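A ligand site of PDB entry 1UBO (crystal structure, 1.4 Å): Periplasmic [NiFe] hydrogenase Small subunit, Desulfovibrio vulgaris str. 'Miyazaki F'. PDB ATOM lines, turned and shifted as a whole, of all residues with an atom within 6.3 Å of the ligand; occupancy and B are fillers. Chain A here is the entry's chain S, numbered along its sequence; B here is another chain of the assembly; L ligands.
O of Gly 149 lies close to S1 of the ligand (3.6 Å).
N of Pro 151 sits close to S2 of the ligand, 3.6 Å away.
Residues that only touch the ligand: Arg 61 of chain B (3.4 Å), Glu 16 (3.7 Å), Gly 112 (3.8 Å), Glu 75 (3.9 Å), Gly 19 (3.9 Å) and Val 120 (3.97 Å).
Hydrophobic or aromatic side chains that line the ligand: Val 120, Pro 151 and His 217 of chain B.
Within 4 Å of the ligand: Glu 16, Cys 17, Gly 19, Cys 20, Glu 75, Gly 112, Thr 113, Cys 114, Val 120, Gly 149, Cys 150, Pro 151, Arg 61 of chain B and His 217 of chain B.
Along chain A the residues within 4 Å of the ligand span positions 16 to 151.
S1 of the ligand lies close to N of Cys 114 (3.4 Å).
SG of Cys 114 is bound to FE2 of the ligand (2.2 Å).
The side-chain sulfur (SG) of Cys 20 binds an iron atom (FE4) of the ligand (2.3 Å).
The backbone NH (N) of Cys 17 lies close to a sulfur (S3) of the ligand.
FE1 of the ligand is bound by SG of Cys 17, at 2.3 Å.
The side-chain sulfur of Cys 150 binds an iron atom (FE3) of the ligand (2.3 Å).
The backbone NH (N) of Thr 113 lies close to a sulfur (S1) of the ligand (3.4 Å).
ND1 of His 217 of chain B lies close to S2 of the ligand (3.7 Å).
The backbone NH of Val 120 sits close to the side-chain sulfur of Cys 114, at 3.7 Å.
NE2 of Gln 121 sits close to SG of Cys 114 (3.3 Å).
The side-chain sulfur (SG) of Cys 20 lies close to the backbone carbonyl oxygen (O) of Tyr 111, at 3.7 Å.
The backbone carbonyl oxygen (O) of Cys 17 is in hydrogen-bond range of the backbone NH (N) of Gly 64 of chain B, 2.8 Å away.
ND1 of His 217 of chain B lies within hydrogen-bond range of O of Cys 150 (3.4 Å).
The side-chain hydroxyl (OG1) of Thr 18 lies within hydrogen-bond range of the side-chain carboxylate (OE1) of Glu 16 (2.6 Å).
The backbone NH (N) of Thr 18 lies close to the side-chain carboxylate (OE1) of Glu 75, at 3.4 Å.
The side-chain carboxylate (OE2) of Glu 75 sits at hydrogen-bond distance from the side-chain hydroxyl (OG) of Ser 21 (2.5 Å).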
ATOM      1  N   ALA A  15     -20.102 -24.282 -29.070  1.00  0.00           N
ATOM      2  CA  ALA A  15     -19.786 -24.196 -27.643  1.00  0.00           C
ATOM      3  C   ALA A  15     -21.105 -23.854 -26.972  1.00  0.00           C
ATOM      4  O   ALA A  15     -21.562 -22.726 -27.030  1.00  0.00           O
ATOM      5  CB  ALA A  15     -18.733 -23.113 -27.364  1.00  0.00           C
ATOM      6  N   GLU A  16     -21.724 -24.864 -26.361  1.00  0.00           N
ATOM      7  CA  GLU A  16     -23.089 -24.802 -25.891  1.00  0.00           C
ATOM      8  C   GLU A  16     -23.300 -25.737 -24.712  1.00  0.00           C
ATOM      9  O   GLU A  16     -22.480 -26.593 -24.403  1.00  0.00           O
ATOM     10  CB  GLU A  16     -24.053 -25.117 -27.054  1.00  0.00           C
ATOM     11  CG  GLU A  16     -23.684 -26.344 -27.883  1.00  0.00           C
ATOM     12  CD  GLU A  16     -24.148 -27.679 -27.323  1.00  0.00           C
ATOM     13  OE1 GLU A  16     -25.268 -27.779 -26.730  1.00  0.00           O
ATOM     14  OE2 GLU A  16     -23.366 -28.651 -27.522  1.00  0.00           O
ATOM     15  N   CYS A  17     -24.408 -25.514 -23.993  1.00  0.00           N
ATOM     16  CA  CYS A  17     -24.757 -26.300 -22.828  1.00  0.00           C
ATOM     17  C   CYS A  17     -25.914 -27.249 -23.127  1.00  0.00           C
ATOM     18  O   CYS A  17     -26.284 -28.036 -22.263  1.00  0.00           O
ATOM     19  CB  CYS A  17     -25.122 -25.410 -21.642  1.00  0.00           C
ATOM     20  SG  CYS A  17     -26.811 -24.732 -21.717  1.00  0.00           S
ATOM     21  N   THR A  18     -26.500 -27.155 -24.286  1.00  0.00           N
ATOM     22  CA  THR A  18     -27.594 -28.018 -24.775  1.00  0.00           C
ATOM     23  C   THR A  18     -28.920 -27.586 -24.181  1.00  0.00           C
ATOM     24  O   THR A  18     -29.966 -28.154 -24.473  1.00  0.00           O
ATOM     25  CB  THR A  18     -27.257 -29.505 -24.627  1.00  0.00           C
ATOM     26  OG1 THR A  18     -25.900 -29.693 -25.102  1.00  0.00           O
ATOM     27  CG2 THR A  18     -28.193 -30.381 -25.453  1.00  0.00           C
ATOM     28  N   GLY A  19     -28.922 -26.485 -23.435  1.00  0.00           N
ATOM     29  CA  GLY A  19     -30.176 -25.877 -22.973  1.00  0.00           C
ATOM     30  C   GLY A  19     -30.988 -25.357 -24.122  1.00  0.00           C
ATOM     31  O   GLY A  19     -32.256 -25.423 -24.030  1.00  0.00           O
ATOM     32  N   CYS A  20     -30.352 -24.861 -25.179  1.00  0.00           N
ATOM     33  CA  CYS A  20     -31.209 -24.408 -26.299  1.00  0.00           C
ATOM     34  C   CYS A  20     -31.828 -25.607 -26.986  1.00  0.00           C
ATOM     35  O   CYS A  20     -33.006 -25.599 -27.372  1.00  0.00           O
ATOM     36  CB  CYS A  20     -30.356 -23.546 -27.239  1.00  0.00           C
ATOM     37  SG  CYS A  20     -29.983 -21.922 -26.583  1.00  0.00           S
ATOM     38  N   SER A  21     -31.082 -26.708 -27.212  1.00  0.00           N
ATOM     39  CA  SER A  21     -31.719 -27.883 -27.771  1.00  0.00           C
ATOM     40  C   SER A  21     -32.879 -28.364 -26.893  1.00  0.00           C
ATOM     41  O   SER A  21     -33.917 -28.739 -27.437  1.00  0.00           O
ATOM     42  CB  SER A  21     -30.775 -29.097 -27.805  1.00  0.00           C
ATOM     43  OG  SER A  21     -29.791 -28.942 -28.821  1.00  0.00           O
ATOM     44  N   GLU A  75     -26.715 -23.667 -32.471  1.00  0.00           N
ATOM     45  CA  GLU A  75     -26.679 -23.469 -31.019  1.00  0.00           C
ATOM     46  C   GLU A  75     -25.237 -23.389 -30.561  1.00  0.00           C
ATOM     47  O   GLU A  75     -24.389 -24.206 -30.990  1.00  0.00           O
ATOM     48  CB  GLU A  75     -27.435 -24.635 -30.345  1.00  0.00           C
ATOM     49  CG  GLU A  75     -27.346 -24.724 -28.810  1.00  0.00           C
ATOM     50  CD  GLU A  75     -28.120 -25.916 -28.264  1.00  0.00           C
ATOM     51  OE1 GLU A  75     -28.194 -25.997 -27.015  1.00  0.00           O
ATOM     52  OE2 GLU A  75     -28.629 -26.696 -29.121  1.00  0.00           O
ATOM     53  N   GLY A  76     -24.893 -22.401 -29.756  1.00  0.00           N
ATOM     54  CA  GLY A  76     -23.576 -22.246 -29.196  1.00  0.00           C
ATOM     55  C   GLY A  76     -22.713 -21.221 -29.922  1.00  0.00           C
ATOM     56  O   GLY A  76     -22.826 -20.959 -31.122  1.00  0.00           O
ATOM     57  N   GLY A  77     -21.776 -20.651 -29.154  1.00  0.00           N
ATOM     58  CA  GLY A  77     -20.773 -19.724 -29.663  1.00  0.00           C
ATOM     59  C   GLY A  77     -19.681 -20.489 -30.394  1.00  0.00           C
ATOM     60  O   GLY A  77     -19.495 -21.681 -30.218  1.00  0.00           O
ATOM     61  N   TYR A 111     -29.599 -19.658 -32.672  1.00  0.00           N
ATOM     62  CA  TYR A 111     -30.593 -19.875 -31.618  1.00  0.00           C
ATOM     63  C   TYR A 111     -29.906 -19.933 -30.259  1.00  0.00           C
ATOM     64  O   TYR A 111     -29.057 -20.817 -30.035  1.00  0.00           O
ATOM     65  CB  TYR A 111     -31.339 -21.189 -31.910  1.00  0.00           C
ATOM     66  CG  TYR A 111     -32.478 -21.452 -30.928  1.00  0.00           C
ATOM     67  CD1 TYR A 111     -33.552 -20.567 -30.812  1.00  0.00           C
ATOM     68  CD2 TYR A 111     -32.464 -22.564 -30.111  1.00  0.00           C
ATOM     69  CE1 TYR A 111     -34.599 -20.776 -29.938  1.00  0.00           C
ATOM     70  CE2 TYR A 111     -33.501 -22.799 -29.218  1.00  0.00           C
ATOM     71  CZ  TYR A 111     -34.559 -21.911 -29.135  1.00  0.00           C
ATOM     72  OH  TYR A 111     -35.603 -22.090 -28.258  1.00  0.00           O
ATOM     73  N   GLY A 112     -30.250 -18.959 -29.419  1.00  0.00           N
ATOM     74  CA  GLY A 112     -29.723 -18.761 -28.094  1.00  0.00           C
ATOM     75  C   GLY A 112     -28.636 -17.688 -28.071  1.00  0.00           C
ATOM     76  O   GLY A 112     -27.919 -17.489 -29.063  1.00  0.00           O
ATOM     77  N   THR A 113     -28.541 -17.016 -26.909  1.00  0.00           N
ATOM     78  CA  THR A 113     -27.580 -15.932 -26.776  1.00  0.00           C
ATOM     79  C   THR A 113     -26.148 -16.363 -27.078  1.00  0.00           C
ATOM     80  O   THR A 113     -25.358 -15.525 -27.533  1.00  0.00           O
ATOM     81  CB  THR A 113     -27.709 -15.391 -25.321  1.00  0.00           C
ATOM     82  OG1 THR A 113     -29.030 -14.802 -25.270  1.00  0.00           O
ATOM     83  CG2 THR A 113     -26.674 -14.317 -24.976  1.00  0.00           C
ATOM     84  N   CYS A 114     -25.762 -17.586 -26.837  1.00  0.00           N
ATOM     85  CA  CYS A 114     -24.393 -17.984 -27.211  1.00  0.00           C
ATOM     86  C   CYS A 114     -24.213 -17.895 -28.721  1.00  0.00           C
ATOM     87  O   CYS A 114     -23.229 -17.291 -29.200  1.00  0.00           O
ATOM     88  CB  CYS A 114     -24.092 -19.423 -26.806  1.00  0.00           C
ATOM     89  SG  CYS A 114     -24.062 -19.696 -24.981  1.00  0.00           S
ATOM     90  N   ALA A 115     -25.143 -18.523 -29.482  1.00  0.00           N
ATOM     91  CA  ALA A 115     -24.969 -18.410 -30.936  1.00  0.00           C
ATOM     92  C   ALA A 115     -25.191 -16.999 -31.426  1.00  0.00           C
ATOM     93  O   ALA A 115     -24.615 -16.563 -32.435  1.00  0.00           O
ATOM     94  CB  ALA A 115     -25.986 -19.320 -31.660  1.00  0.00           C
ATOM     95  N   GLY A 119     -22.334 -15.355 -25.723  1.00  0.00           N
ATOM     96  CA  GLY A 119     -22.866 -16.071 -24.581  1.00  0.00           C
ATOM     97  C   GLY A 119     -21.879 -16.341 -23.459  1.00  0.00           C
ATOM     98  O   GLY A 119     -20.877 -15.656 -23.274  1.00  0.00           O
ATOM     99  N   VAL A 120     -22.179 -17.414 -22.679  1.00  0.00           N
ATOM    100  CA  VAL A 120     -21.529 -17.558 -21.380  1.00  0.00           C
ATOM    101  C   VAL A 120     -20.032 -17.758 -21.569  1.00  0.00           C
ATOM    102  O   VAL A 120     -19.257 -17.212 -20.756  1.00  0.00           O
ATOM    103  CB  VAL A 120     -22.175 -18.694 -20.546  1.00  0.00           C
ATOM    104  CG1 VAL A 120     -21.928 -20.075 -21.168  1.00  0.00           C
ATOM    105  CG2 VAL A 120     -21.725 -18.663 -19.092  1.00  0.00           C
ATOM    106  N   GLN A 121     -19.583 -18.523 -22.561  1.00  0.00           N
ATOM    107  CA  GLN A 121     -18.128 -18.747 -22.671  1.00  0.00           C
ATOM    108  C   GLN A 121     -17.455 -17.509 -23.232  1.00  0.00           C
ATOM    109  O   GLN A 121     -16.213 -17.413 -23.156  1.00  0.00           O
ATOM    110  CB  GLN A 121     -17.825 -19.950 -23.550  1.00  0.00           C
ATOM    111  CG  GLN A 121     -18.419 -19.979 -24.966  1.00  0.00           C
ATOM    112  CD  GLN A 121     -19.835 -20.463 -24.954  1.00  0.00           C
ATOM    113  OE1 GLN A 121     -20.158 -21.490 -24.313  1.00  0.00           O
ATOM    114  NE2 GLN A 121     -20.775 -19.784 -25.579  1.00  0.00           N
ATOM    115  N   GLY A 149     -31.790 -15.302 -25.942  1.00  0.00           N
ATOM    116  CA  GLY A 149     -32.250 -15.787 -24.657  1.00  0.00           C
ATOM    117  C   GLY A 149     -31.384 -16.987 -24.259  1.00  0.00           C
ATOM    118  O   GLY A 149     -30.727 -17.621 -25.107  1.00  0.00           O
ATOM    119  N   CYS A 150     -31.451 -17.338 -22.964  1.00  0.00           N
ATOM    120  CA  CYS A 150     -30.503 -18.341 -22.434  1.00  0.00           C
ATOM    121  C   CYS A 150     -31.221 -19.355 -21.573  1.00  0.00           C
ATOM    122  O   CYS A 150     -31.069 -19.403 -20.330  1.00  0.00           O
ATOM    123  CB  CYS A 150     -29.400 -17.586 -21.664  1.00  0.00           C
ATOM    124  SG  CYS A 150     -27.949 -18.601 -21.247  1.00  0.00           S
ATOM    125  N   PRO A 151     -32.019 -20.245 -22.196  1.00  0.00           N
ATOM    126  CA  PRO A 151     -32.303 -20.307 -23.628  1.00  0.00           C
ATOM    127  C   PRO A 151     -33.504 -19.456 -24.036  1.00  0.00           C
ATOM    128  O   PRO A 151     -34.254 -18.935 -23.187  1.00  0.00           O
ATOM    129  CB  PRO A 151     -32.634 -21.796 -23.812  1.00  0.00           C
ATOM    130  CG  PRO A 151     -33.381 -22.110 -22.507  1.00  0.00           C
ATOM    131  CD  PRO A 151     -32.667 -21.356 -21.411  1.00  0.00           C
ATOM    132  N   PRO A 152     -33.692 -19.257 -25.333  1.00  0.00           N
ATOM    133  CA  PRO A 152     -34.817 -18.466 -25.837  1.00  0.00           C
ATOM    134  C   PRO A 152     -36.106 -19.199 -25.544  1.00  0.00           C
ATOM    135  O   PRO A 152     -36.127 -20.395 -25.224  1.00  0.00           O
ATOM    136  CB  PRO A 152     -34.625 -18.416 -27.376  1.00  0.00           C
ATOM    137  CG  PRO A 152     -33.163 -18.788 -27.559  1.00  0.00           C
ATOM    138  CD  PRO A 152     -32.887 -19.787 -26.448  1.00  0.00           C
ATOM    139  N   TRP A 258     -23.702 -11.390 -19.554  1.00  0.00           N
ATOM    140  CA  TRP A 258     -22.929 -11.876 -18.405  1.00  0.00           C
ATOM    141  C   TRP A 258     -22.043 -10.798 -17.783  1.00  0.00           C
ATOM    142  O   TRP A 258     -21.753 -10.839 -16.581  1.00  0.00           O
ATOM    143  CB  TRP A 258     -22.060 -13.029 -18.915  1.00  0.00           C
ATOM    144  CG  TRP A 258     -22.931 -14.155 -19.388  1.00  0.00           C
ATOM    145  CD1 TRP A 258     -23.184 -14.498 -20.698  1.00  0.00           C
ATOM    146  CD2 TRP A 258     -23.674 -15.048 -18.584  1.00  0.00           C
ATOM    147  NE1 TRP A 258     -24.043 -15.580 -20.747  1.00  0.00           N
ATOM    148  CE2 TRP A 258     -24.351 -15.928 -19.456  1.00  0.00           C
ATOM    149  CE3 TRP A 258     -23.821 -15.197 -17.191  1.00  0.00           C
ATOM    150  CZ2 TRP A 258     -25.202 -16.976 -19.015  1.00  0.00           C
ATOM    151  CZ3 TRP A 258     -24.654 -16.217 -16.747  1.00  0.00           C
ATOM    152  CH2 TRP A 258     -25.321 -17.081 -17.635  1.00  0.00           C
ATOM    153  N   ARG B  41     -14.919 -24.682 -22.435  1.00  0.00           N
ATOM    154  CA  ARG B  41     -15.468 -23.338 -22.276  1.00  0.00           C
ATOM    155  C   ARG B  41     -14.738 -22.531 -21.215  1.00  0.00           C
ATOM    156  O   ARG B  41     -14.550 -21.322 -21.411  1.00  0.00           O
ATOM    157  CB  ARG B  41     -16.969 -23.408 -21.968  1.00  0.00           C
ATOM    158  CG  ARG B  41     -17.744 -23.847 -23.217  1.00  0.00           C
ATOM    159  CD  ARG B  41     -19.253 -24.087 -23.017  1.00  0.00           C
ATOM    160  NE  ARG B  41     -19.404 -25.134 -22.024  1.00  0.00           N
ATOM    161  CZ  ARG B  41     -20.390 -25.315 -21.177  1.00  0.00           C
ATOM    162  NH1 ARG B  41     -21.461 -24.522 -21.202  1.00  0.00           N
ATOM    163  NH2 ARG B  41     -20.365 -26.306 -20.291  1.00  0.00           N
ATOM    164  N   ARG B  61     -25.348 -22.633 -16.520  1.00  0.00           N
ATOM    165  CA  ARG B  61     -25.081 -22.797 -17.966  1.00  0.00           C
ATOM    166  C   ARG B  61     -23.922 -23.758 -18.256  1.00  0.00           C
ATOM    167  O   ARG B  61     -23.491 -23.925 -19.398  1.00  0.00           O
ATOM    168  CB  ARG B  61     -24.844 -21.436 -18.621  1.00  0.00           C
ATOM    169  CG  ARG B  61     -26.139 -20.717 -18.909  1.00  0.00           C
ATOM    170  CD  ARG B  61     -26.910 -20.314 -17.653  1.00  0.00           C
ATOM    171  NE  ARG B  61     -28.101 -19.582 -18.131  1.00  0.00           N
ATOM    172  CZ  ARG B  61     -29.000 -19.065 -17.294  1.00  0.00           C
ATOM    173  NH1 ARG B  61     -28.766 -19.173 -15.991  1.00  0.00           N
ATOM    174  NH2 ARG B  61     -30.080 -18.486 -17.789  1.00  0.00           N
ATOM    175  N   GLY B  64     -27.635 -27.581 -19.846  1.00  0.00           N
ATOM    176  CA  GLY B  64     -29.081 -27.422 -19.935  1.00  0.00           C
ATOM    177  C   GLY B  64     -29.823 -28.745 -20.048  1.00  0.00           C
ATOM    178  O   GLY B  64     -31.051 -28.708 -20.068  1.00  0.00           O
ATOM    179  N   PRO B 216     -35.828 -24.947 -19.865  1.00  0.00           N
ATOM    180  CA  PRO B 216     -34.591 -25.024 -19.116  1.00  0.00           C
ATOM    181  C   PRO B 216     -34.170 -23.741 -18.415  1.00  0.00           C
ATOM    182  O   PRO B 216     -34.592 -22.615 -18.753  1.00  0.00           O
ATOM    183  CB  PRO B 216     -33.494 -25.311 -20.202  1.00  0.00           C
ATOM    184  CG  PRO B 216     -34.295 -25.902 -21.316  1.00  0.00           C
ATOM    185  CD  PRO B 216     -35.551 -25.041 -21.321  1.00  0.00           C
ATOM    186  N   HIS B 217     -33.297 -23.943 -17.418  1.00  0.00           N
ATOM    187  CA  HIS B 217     -32.534 -22.980 -16.630  1.00  0.00           C
ATOM    188  C   HIS B 217     -33.481 -22.235 -15.692  1.00  0.00           C
ATOM    189  O   HIS B 217     -34.019 -21.160 -15.976  1.00  0.00           O
ATOM    190  CB  HIS B 217     -31.714 -22.026 -17.523  1.00  0.00           C
ATOM    191  CG  HIS B 217     -30.540 -22.763 -18.116  1.00  0.00           C
ATOM    192  ND1 HIS B 217     -29.775 -22.371 -19.162  1.00  0.00           N
ATOM    193  CD2 HIS B 217     -30.049 -23.969 -17.660  1.00  0.00           C
ATOM    194  CE1 HIS B 217     -28.813 -23.331 -19.361  1.00  0.00           C
ATOM    195  NE2 HIS B 217     -29.019 -24.275 -18.450  1.00  0.00           N
HETATM  196 FE1  LIG L   1     -26.862 -22.846 -23.014  1.00  0.00          FE
HETATM  197 FE2  LIG L   1     -25.883 -20.911 -24.528  1.00  0.00          FE
HETATM  198 FE3  LIG L   1     -27.731 -20.342 -22.734  1.00  0.00          FE
HETATM  199 FE4  LIG L   1     -28.426 -21.804 -24.938  1.00  0.00          FE
HETATM  200  S1  LIG L   1     -27.744 -19.626 -24.925  1.00  0.00           S
HETATM  201  S2  LIG L   1     -29.047 -22.130 -22.775  1.00  0.00           S
HETATM  202  S3  LIG L   1     -26.455 -22.978 -25.300  1.00  0.00           S
HETATM  203  S4  LIG L   1     -25.592 -21.150 -22.271  1.00  0.00           S
